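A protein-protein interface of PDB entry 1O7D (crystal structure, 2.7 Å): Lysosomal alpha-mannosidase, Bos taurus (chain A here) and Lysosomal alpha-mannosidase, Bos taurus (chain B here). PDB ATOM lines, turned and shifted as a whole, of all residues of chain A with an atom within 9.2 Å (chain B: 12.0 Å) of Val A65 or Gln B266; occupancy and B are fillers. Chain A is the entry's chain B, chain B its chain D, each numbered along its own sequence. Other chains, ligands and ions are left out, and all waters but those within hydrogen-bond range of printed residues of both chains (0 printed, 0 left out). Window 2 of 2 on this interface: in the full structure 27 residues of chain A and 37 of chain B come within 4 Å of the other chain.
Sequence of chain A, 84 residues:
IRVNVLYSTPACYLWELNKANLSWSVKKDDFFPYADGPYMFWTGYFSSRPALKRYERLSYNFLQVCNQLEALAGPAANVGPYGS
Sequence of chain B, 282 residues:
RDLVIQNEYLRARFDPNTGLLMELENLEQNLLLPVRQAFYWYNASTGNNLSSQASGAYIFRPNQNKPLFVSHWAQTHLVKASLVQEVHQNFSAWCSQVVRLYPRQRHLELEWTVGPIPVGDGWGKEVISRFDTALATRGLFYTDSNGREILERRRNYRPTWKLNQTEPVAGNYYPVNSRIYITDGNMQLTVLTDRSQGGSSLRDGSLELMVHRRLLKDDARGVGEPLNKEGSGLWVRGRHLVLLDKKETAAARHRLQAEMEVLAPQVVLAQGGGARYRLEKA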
ATOM      1  N   LEU A  58     -17.772  10.734 -28.643  1.00  0.00           N
ATOM      2  CA  LEU A  58     -19.143  11.213 -28.698  1.00  0.00           C
ATOM      3  C   LEU A  58     -19.877  10.716 -27.471  1.00  0.00           C
ATOM      4  O   LEU A  58     -20.672  11.444 -26.876  1.00  0.00           O
ATOM      5  CB  LEU A  58     -19.828  10.695 -29.954  1.00  0.00           C
ATOM      6  CG  LEU A  58     -21.323  10.967 -30.121  1.00  0.00           C
ATOM      7  CD1 LEU A  58     -21.579  12.461 -30.191  1.00  0.00           C
ATOM      8  CD2 LEU A  58     -21.812  10.257 -31.385  1.00  0.00           C
ATOM      9  N   SER A  59     -19.613   9.470 -27.092  1.00  0.00           N
ATOM     10  CA  SER A  59     -20.256   8.906 -25.914  1.00  0.00           C
ATOM     11  C   SER A  59     -19.842   9.734 -24.684  1.00  0.00           C
ATOM     12  O   SER A  59     -20.585   9.826 -23.685  1.00  0.00           O
ATOM     13  CB  SER A  59     -19.860   7.438 -25.740  1.00  0.00           C
ATOM     14  OG  SER A  59     -20.364   6.640 -26.790  1.00  0.00           O
ATOM     15  N   TYR A  60     -18.657  10.340 -24.763  1.00  0.00           N
ATOM     16  CA  TYR A  60     -18.176  11.178 -23.675  1.00  0.00           C
ATOM     17  C   TYR A  60     -19.120  12.381 -23.511  1.00  0.00           C
ATOM     18  O   TYR A  60     -19.666  12.624 -22.430  1.00  0.00           O
ATOM     19  CB  TYR A  60     -16.757  11.682 -23.961  1.00  0.00           C
ATOM     20  CG  TYR A  60     -16.250  12.652 -22.903  1.00  0.00           C
ATOM     21  CD1 TYR A  60     -15.746  12.192 -21.680  1.00  0.00           C
ATOM     22  CD2 TYR A  60     -16.310  14.033 -23.114  1.00  0.00           C
ATOM     23  CE1 TYR A  60     -15.318  13.084 -20.703  1.00  0.00           C
ATOM     24  CE2 TYR A  60     -15.886  14.929 -22.143  1.00  0.00           C
ATOM     25  CZ  TYR A  60     -15.390  14.453 -20.941  1.00  0.00           C
ATOM     26  OH  TYR A  60     -14.959  15.350 -19.990  1.00  0.00           O
ATOM     27  N   ASN A  61     -19.302  13.125 -24.599  1.00  0.00           N
ATOM     28  CA  ASN A  61     -20.162  14.297 -24.616  1.00  0.00           C
ATOM     29  C   ASN A  61     -21.506  13.904 -24.058  1.00  0.00           C
ATOM     30  O   ASN A  61     -22.129  14.660 -23.321  1.00  0.00           O
ATOM     31  CB  ASN A  61     -20.344  14.789 -26.052  1.00  0.00           C
ATOM     32  CG  ASN A  61     -20.947  16.174 -26.125  1.00  0.00           C
ATOM     33  OD1 ASN A  61     -21.100  16.746 -27.205  1.00  0.00           O
ATOM     34  ND2 ASN A  61     -21.282  16.725 -24.975  1.00  0.00           N
ATOM     35  N   PHE A  62     -21.928  12.696 -24.417  1.00  0.00           N
ATOM     36  CA  PHE A  62     -23.216  12.159 -24.013  1.00  0.00           C
ATOM     37  C   PHE A  62     -23.301  11.796 -22.534  1.00  0.00           C
ATOM     38  O   PHE A  62     -24.249  12.192 -21.854  1.00  0.00           O
ATOM     39  CB  PHE A  62     -23.561  10.939 -24.880  1.00  0.00           C
ATOM     40  CG  PHE A  62     -24.980  10.460 -24.720  1.00  0.00           C
ATOM     41  CD1 PHE A  62     -26.041  11.246 -25.144  1.00  0.00           C
ATOM     42  CD2 PHE A  62     -25.255   9.243 -24.104  1.00  0.00           C
ATOM     43  CE1 PHE A  62     -27.359  10.828 -24.953  1.00  0.00           C
ATOM     44  CE2 PHE A  62     -26.573   8.810 -23.907  1.00  0.00           C
ATOM     45  CZ  PHE A  62     -27.625   9.603 -24.328  1.00  0.00           C
ATOM     46  N   LEU A  63     -22.327  11.039 -22.042  1.00  0.00           N
ATOM     47  CA  LEU A  63     -22.316  10.647 -20.638  1.00  0.00           C
ATOM     48  C   LEU A  63     -22.351  11.909 -19.763  1.00  0.00           C
ATOM     49  O   LEU A  63     -23.024  11.957 -18.731  1.00  0.00           O
ATOM     50  CB  LEU A  63     -21.044   9.853 -20.335  1.00  0.00           C
ATOM     51  CG  LEU A  63     -20.967   8.851 -19.175  1.00  0.00           C
ATOM     52  CD1 LEU A  63     -19.523   8.806 -18.715  1.00  0.00           C
ATOM     53  CD2 LEU A  63     -21.860   9.236 -18.027  1.00  0.00           C
ATOM     54  N   GLN A  64     -21.610  12.924 -20.188  1.00  0.00           N
ATOM     55  CA  GLN A  64     -21.540  14.192 -19.479  1.00  0.00           C
ATOM     56  C   GLN A  64     -22.931  14.777 -19.309  1.00  0.00           C
ATOM     57  O   GLN A  64     -23.366  15.062 -18.197  1.00  0.00           O
ATOM     58  CB  GLN A  64     -20.689  15.175 -20.264  1.00  0.00           C
ATOM     59  CG  GLN A  64     -19.703  15.883 -19.401  1.00  0.00           C
ATOM     60  CD  GLN A  64     -18.531  15.005 -19.053  1.00  0.00           C
ATOM     61  OE1 GLN A  64     -18.691  13.826 -18.696  1.00  0.00           O
ATOM     62  NE2 GLN A  64     -17.334  15.574 -19.145  1.00  0.00           N
ATOM     63  N   VAL A  65     -23.607  14.979 -20.433  1.00  0.00           N
ATOM     64  CA  VAL A  65     -24.953  15.506 -20.436  1.00  0.00           C
ATOM     65  C   VAL A  65     -25.791  14.636 -19.525  1.00  0.00           C
ATOM     66  O   VAL A  65     -26.581  15.132 -18.747  1.00  0.00           O
ATOM     67  CB  VAL A  65     -25.529  15.474 -21.858  1.00  0.00           C
ATOM     68  CG1 VAL A  65     -26.979  15.869 -21.846  1.00  0.00           C
ATOM     69  CG2 VAL A  65     -24.725  16.416 -22.758  1.00  0.00           C
ATOM     70  N   CYS A  66     -25.603  13.326 -19.618  1.00  0.00           N
ATOM     71  CA  CYS A  66     -26.336  12.381 -18.777  1.00  0.00           C
ATOM     72  C   CYS A  66     -26.038  12.698 -17.308  1.00  0.00           C
ATOM     73  O   CYS A  66     -26.957  12.817 -16.499  1.00  0.00           O
ATOM     74  CB  CYS A  66     -25.921  10.933 -19.118  1.00  0.00           C
ATOM     75  SG  CYS A  66     -26.823   9.539 -18.306  1.00  0.00           S
ATOM     76  N   ASN A  67     -24.757  12.847 -16.971  1.00  0.00           N
ATOM     77  CA  ASN A  67     -24.357  13.161 -15.604  1.00  0.00           C
ATOM     78  C   ASN A  67     -24.975  14.453 -15.106  1.00  0.00           C
ATOM     79  O   ASN A  67     -25.603  14.476 -14.046  1.00  0.00           O
ATOM     80  CB  ASN A  67     -22.839  13.282 -15.493  1.00  0.00           C
ATOM     81  CG  ASN A  67     -22.163  11.943 -15.384  1.00  0.00           C
ATOM     82  OD1 ASN A  67     -22.636  11.062 -14.662  1.00  0.00           O
ATOM     83  ND2 ASN A  67     -21.050  11.778 -16.089  1.00  0.00           N
ATOM     84  N   GLN A  68     -24.791  15.532 -15.866  1.00  0.00           N
ATOM     85  CA  GLN A  68     -25.322  16.830 -15.478  1.00  0.00           C
ATOM     86  C   GLN A  68     -26.811  16.788 -15.213  1.00  0.00           C
ATOM     87  O   GLN A  68     -27.276  17.447 -14.303  1.00  0.00           O
ATOM     88  CB  GLN A  68     -25.060  17.887 -16.544  1.00  0.00           C
ATOM     89  CG  GLN A  68     -23.620  18.211 -16.832  1.00  0.00           C
ATOM     90  CD  GLN A  68     -23.461  19.565 -17.541  1.00  0.00           C
ATOM     91  OE1 GLN A  68     -24.391  20.071 -18.179  1.00  0.00           O
ATOM     92  NE2 GLN A  68     -22.278  20.145 -17.435  1.00  0.00           N
ATOM     93  N   LEU A  69     -27.571  16.028 -15.996  1.00  0.00           N
ATOM     94  CA  LEU A  69     -29.016  15.983 -15.772  1.00  0.00           C
ATOM     95  C   LEU A  69     -29.431  15.204 -14.523  1.00  0.00           C
ATOM     96  O   LEU A  69     -30.406  15.558 -13.845  1.00  0.00           O
ATOM     97  CB  LEU A  69     -29.738  15.412 -16.999  1.00  0.00           C
ATOM     98  CG  LEU A  69     -30.020  16.423 -18.109  1.00  0.00           C
ATOM     99  CD1 LEU A  69     -30.790  15.742 -19.215  1.00  0.00           C
ATOM    100  CD2 LEU A  69     -30.803  17.594 -17.549  1.00  0.00           C
ATOM    101  N   GLU A  70     -28.691  14.139 -14.233  1.00  0.00           N
ATOM    102  CA  GLU A  70     -28.955  13.304 -13.073  1.00  0.00           C
ATOM    103  C   GLU A  70     -28.692  14.162 -11.836  1.00  0.00           C
ATOM    104  O   GLU A  70     -29.352  14.015 -10.811  1.00  0.00           O
ATOM    105  CB  GLU A  70     -28.012  12.098 -13.107  1.00  0.00           C
ATOM    106  CG  GLU A  70     -28.221  11.047 -12.027  1.00  0.00           C
ATOM    107  CD  GLU A  70     -27.242   9.870 -12.164  1.00  0.00           C
ATOM    108  OE1 GLU A  70     -26.023  10.112 -12.324  1.00  0.00           O
ATOM    109  OE2 GLU A  70     -27.685   8.699 -12.107  1.00  0.00           O
ATOM    110  N   ALA A  71     -27.733  15.076 -11.958  1.00  0.00           N
ATOM    111  CA  ALA A  71     -27.358  15.963 -10.867  1.00  0.00           C
ATOM    112  C   ALA A  71     -28.405  17.032 -10.612  1.00  0.00           C
ATOM    113  O   ALA A  71     -28.721  17.346  -9.468  1.00  0.00           O
ATOM    114  CB  ALA A  71     -26.004  16.615 -11.169  1.00  0.00           C
ATOM    115  N   LEU A  72     -28.938  17.600 -11.684  1.00  0.00           N
ATOM    116  CA  LEU A  72     -29.957  18.637 -11.573  1.00  0.00           C
ATOM    117  C   LEU A  72     -31.318  18.102 -11.073  1.00  0.00           C
ATOM    118  O   LEU A  72     -32.050  18.814 -10.387  1.00  0.00           O
ATOM    119  CB  LEU A  72     -30.107  19.347 -12.921  1.00  0.00           C
ATOM    120  CG  LEU A  72     -28.796  19.954 -13.429  1.00  0.00           C
ATOM    121  CD1 LEU A  72     -29.001  20.616 -14.783  1.00  0.00           C
ATOM    122  CD2 LEU A  72     -28.283  20.945 -12.415  1.00  0.00           C
ATOM    123  N   ALA A  73     -31.659  16.857 -11.406  1.00  0.00           N
ATOM    124  CA  ALA A  73     -32.918  16.268 -10.927  1.00  0.00           C
ATOM    125  C   ALA A  73     -32.637  15.585  -9.584  1.00  0.00           C
ATOM    126  O   ALA A  73     -31.530  15.075  -9.377  1.00  0.00           O
ATOM    127  CB  ALA A  73     -33.437  15.247 -11.935  1.00  0.00           C
ATOM    128  N   ARG B 239     -15.750  15.918 -39.199  1.00  0.00           N
ATOM    129  CA  ARG B 239     -15.595  17.362 -39.419  1.00  0.00           C
ATOM    130  C   ARG B 239     -14.228  17.883 -38.969  1.00  0.00           C
ATOM    131  O   ARG B 239     -13.565  17.282 -38.125  1.00  0.00           O
ATOM    132  CB  ARG B 239     -16.691  18.149 -38.684  1.00  0.00           C
ATOM    133  CG  ARG B 239     -18.091  17.557 -38.814  1.00  0.00           C
ATOM    134  CD  ARG B 239     -19.180  18.539 -38.408  1.00  0.00           C
ATOM    135  NE  ARG B 239     -18.884  19.245 -37.164  1.00  0.00           N
ATOM    136  CZ  ARG B 239     -18.668  18.667 -35.979  1.00  0.00           C
ATOM    137  NH1 ARG B 239     -18.708  17.344 -35.830  1.00  0.00           N
ATOM    138  NH2 ARG B 239     -18.406  19.428 -34.927  1.00  0.00           N
ATOM    139  N   GLU B 259     -13.716  23.645 -26.718  1.00  0.00           N
ATOM    140  CA  GLU B 259     -14.571  23.145 -25.654  1.00  0.00           C
ATOM    141  C   GLU B 259     -16.021  23.031 -26.125  1.00  0.00           C
ATOM    142  O   GLU B 259     -16.744  22.142 -25.683  1.00  0.00           O
ATOM    143  CB  GLU B 259     -14.497  24.023 -24.404  1.00  0.00           C
ATOM    144  CG  GLU B 259     -14.912  25.435 -24.608  1.00  0.00           C
ATOM    145  CD  GLU B 259     -15.625  26.032 -23.376  1.00  0.00           C
ATOM    146  OE1 GLU B 259     -15.622  25.397 -22.267  1.00  0.00           O
ATOM    147  OE2 GLU B 259     -16.184  27.155 -23.542  1.00  0.00           O
ATOM    148  N   MET B 260     -16.454  23.912 -27.021  1.00  0.00           N
ATOM    149  CA  MET B 260     -17.825  23.840 -27.512  1.00  0.00           C
ATOM    150  C   MET B 260     -17.973  22.616 -28.397  1.00  0.00           C
ATOM    151  O   MET B 260     -19.077  22.150 -28.662  1.00  0.00           O
ATOM    152  CB  MET B 260     -18.186  25.087 -28.310  1.00  0.00           C
ATOM    153  CG  MET B 260     -18.302  26.339 -27.478  1.00  0.00           C
ATOM    154  SD  MET B 260     -18.955  27.730 -28.453  1.00  0.00           S
ATOM    155  CE  MET B 260     -17.446  28.603 -28.946  1.00  0.00           C
ATOM    156  N   GLU B 261     -16.832  22.092 -28.824  1.00  0.00           N
ATOM    157  CA  GLU B 261     -16.742  20.930 -29.698  1.00  0.00           C
ATOM    158  C   GLU B 261     -16.903  19.584 -28.982  1.00  0.00           C
ATOM    159  O   GLU B 261     -17.579  18.686 -29.478  1.00  0.00           O
ATOM    160  CB  GLU B 261     -15.393  20.984 -30.420  1.00  0.00           C
ATOM    161  CG  GLU B 261     -15.199  19.980 -31.532  1.00  0.00           C
ATOM    162  CD  GLU B 261     -16.367  19.945 -32.475  1.00  0.00           C
ATOM    163  OE1 GLU B 261     -16.843  21.036 -32.877  1.00  0.00           O
ATOM    164  OE2 GLU B 261     -16.805  18.822 -32.808  1.00  0.00           O
ATOM    165  N   VAL B 262     -16.259  19.436 -27.829  1.00  0.00           N
ATOM    166  CA  VAL B 262     -16.356  18.206 -27.052  1.00  0.00           C
ATOM    167  C   VAL B 262     -17.618  18.192 -26.164  1.00  0.00           C
ATOM    168  O   VAL B 262     -18.301  17.169 -26.052  1.00  0.00           O
ATOM    169  CB  VAL B 262     -15.097  18.025 -26.187  1.00  0.00           C
ATOM    170  CG1 VAL B 262     -15.183  16.737 -25.361  1.00  0.00           C
ATOM    171  CG2 VAL B 262     -13.885  17.975 -27.093  1.00  0.00           C
ATOM    172  N   LEU B 263     -17.919  19.324 -25.531  1.00  0.00           N
ATOM    173  CA  LEU B 263     -19.100  19.443 -24.682  1.00  0.00           C
ATOM    174  C   LEU B 263     -20.165  20.147 -25.496  1.00  0.00           C
ATOM    175  O   LEU B 263     -20.610  21.238 -25.147  1.00  0.00           O
ATOM    176  CB  LEU B 263     -18.772  20.252 -23.438  1.00  0.00           C
ATOM    177  CG  LEU B 263     -17.915  19.473 -22.453  1.00  0.00           C
ATOM    178  CD1 LEU B 263     -17.651  20.316 -21.217  1.00  0.00           C
ATOM    179  CD2 LEU B 263     -18.652  18.181 -22.098  1.00  0.00           C
ATOM    180  N   ALA B 264     -20.559  19.514 -26.594  1.00  0.00           N
ATOM    181  CA  ALA B 264     -21.543  20.076 -27.499  1.00  0.00           C
ATOM    182  C   ALA B 264     -22.969  19.919 -26.986  1.00  0.00           C
ATOM    183  O   ALA B 264     -23.210  19.238 -25.994  1.00  0.00           O
ATOM    184  CB  ALA B 264     -21.393  19.431 -28.853  1.00  0.00           C
ATOM    185  N   PRO B 265     -23.936  20.560 -27.658  1.00  0.00           N
ATOM    186  CA  PRO B 265     -25.316  20.438 -27.195  1.00  0.00           C
ATOM    187  C   PRO B 265     -25.973  19.111 -27.578  1.00  0.00           C
ATOM    188  O   PRO B 265     -25.629  18.517 -28.596  1.00  0.00           O
ATOM    189  CB  PRO B 265     -25.983  21.666 -27.807  1.00  0.00           C
ATOM    190  CG  PRO B 265     -25.239  21.861 -29.052  1.00  0.00           C
ATOM    191  CD  PRO B 265     -23.815  21.604 -28.689  1.00  0.00           C
ATOM    192  N   GLN B 266     -26.893  18.640 -26.732  1.00  0.00           N
ATOM    193  CA  GLN B 266     -27.614  17.395 -26.959  1.00  0.00           C
ATOM    194  C   GLN B 266     -29.065  17.714 -27.350  1.00  0.00           C
ATOM    195  O   GLN B 266     -29.700  18.607 -26.784  1.00  0.00           O
ATOM    196  CB  GLN B 266     -27.579  16.536 -25.692  1.00  0.00           C
ATOM    197  CG  GLN B 266     -28.382  15.244 -25.754  1.00  0.00           C
ATOM    198  CD  GLN B 266     -27.879  14.297 -26.825  1.00  0.00           C
ATOM    199  OE1 GLN B 266     -26.670  14.120 -26.987  1.00  0.00           O
ATOM    200  NE2 GLN B 266     -28.811  13.669 -27.560  1.00  0.00           N
ATOM    201  N   VAL B 267     -29.581  16.994 -28.335  1.00  0.00           N
ATOM    202  CA  VAL B 267     -30.932  17.220 -28.783  1.00  0.00           C
ATOM    203  C   VAL B 267     -31.790  16.013 -28.529  1.00  0.00           C
ATOM    204  O   VAL B 267     -31.381  14.886 -28.811  1.00  0.00           O
ATOM    205  CB  VAL B 267     -30.966  17.520 -30.259  1.00  0.00           C
ATOM    206  CG1 VAL B 267     -32.346  17.272 -30.805  1.00  0.00           C
ATOM    207  CG2 VAL B 267     -30.558  18.938 -30.483  1.00  0.00           C
ATOM    208  N   VAL B 268     -32.975  16.265 -27.973  1.00  0.00           N
ATOM    209  CA  VAL B 268     -33.953  15.225 -27.679  1.00  0.00           C
ATOM    210  C   VAL B 268     -35.293  15.725 -28.219  1.00  0.00           C
ATOM    211  O   VAL B 268     -35.643  16.901 -28.071  1.00  0.00           O
ATOM    212  CB  VAL B 268     -34.067  14.927 -26.159  1.00  0.00           C
ATOM    213  CG1 VAL B 268     -34.591  16.135 -25.437  1.00  0.00           C
ATOM    214  CG2 VAL B 268     -34.983  13.734 -25.923  1.00  0.00           C
ATOM    215  N   LEU B 269     -36.037  14.824 -28.847  1.00  0.00           N
ATOM    216  CA  LEU B 269     -37.300  15.192 -29.439  1.00  0.00           C
ATOM    217  C   LEU B 269     -38.484  14.622 -28.715  1.00  0.00           C
ATOM    218  O   LEU B 269     -38.387  13.605 -28.031  1.00  0.00           O
ATOM    219  CB  LEU B 269     -37.329  14.739 -30.890  1.00  0.00           C
ATOM    220  CG  LEU B 269     -36.029  15.034 -31.632  1.00  0.00           C
ATOM    221  CD1 LEU B 269     -36.106  14.431 -33.027  1.00  0.00           C
ATOM    222  CD2 LEU B 269     -35.784  16.537 -31.680  1.00  0.00           C
ATOM    223  N   ALA B 270     -39.609  15.303 -28.891  1.00  0.00           N
ATOM    224  CA  ALA B 270     -40.875  14.919 -28.293  1.00  0.00           C
ATOM    225  C   ALA B 270     -41.987  15.329 -29.256  1.00  0.00           C
ATOM    226  O   ALA B 270     -41.997  16.446 -29.789  1.00  0.00           O
ATOM    227  CB  ALA B 270     -41.053  15.616 -26.954  1.00  0.00           C
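The side-chain amide nitrogen of Gln A64 is in hydrogen-bond range of the side-chain hydroxyl of Tyr A60 (2.5 Å).
Among the printed residues, merely in contact across the chains: Phe A62 with Gln B266 (3.5 Å), Asn A61 with Leu B263 (3.5 Å), Tyr A60 with Val B262 (3.7 Å), Gln A64 with Leu B263 (3.7 Å) and Val A65 with Gln B266 (3.9 Å).
The side-chain amide oxygen (OD1) of Asn A61 sits close to the backbone carbonyl oxygen (O) of Val B262 (3.1 Å).
OD1 of Asn A61 lies within hydrogen-bond range of N of Ala B264 (2.9 Å).
Of the 16 printed residues of chain A, 5 touch a printed residue of chain B.
Printed residues of chain A that touch a printed residue of chain B: Tyr A60, Asn A61, Phe A62, Gln A64 and Val A65.
Printed residues of chain B that touch a printed residue of chain A: Val B262, Leu B263, Ala B264 and Gln B266.
Among the printed residues, 7 pairs touch across the chains.
Leu A58 touches none of the printed residues of chain B.
Of the printed residues of chain B, Tyr A60 touches Val B262 (3.7 Å).
Asn A61 touches just these residues of chain B: Val B262, Leu B263 and Ala B264.
Of chain B, only Gln B266 (3.5 Å) comes within 4 Å of Phe A62.
Of chain B, only Leu B263 comes within 4 Å of Gln A64.
No residue of chain B comes within 4 Å of Cys A66.
No residue of chain B comes within 4 Å of Gln A68.
Printed residues of chain A within 4 Å of Val B262: Tyr A60 and Asn A61.
Printed residues of chain A within 4 Å of Leu B263: Asn A61 and Gln A64.
Printed residues of chain A within 4 Å of Ala B264: Asn A61.
Gln B266 touches just these residues of chain A: Phe A62 and Val A65.
No residue of chain A comes within 4 Å of Val B267.
The nearest residue of chain B that does not touch Val A65 is Ala B264 (4.6 Å).
The nearest residue of chain A that does not touch Gln B266 is Asn A61 (5.9 Å).
The nearest printed residue of chain A that does not touch Ala B264 is Val A65 (4.6 Å).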
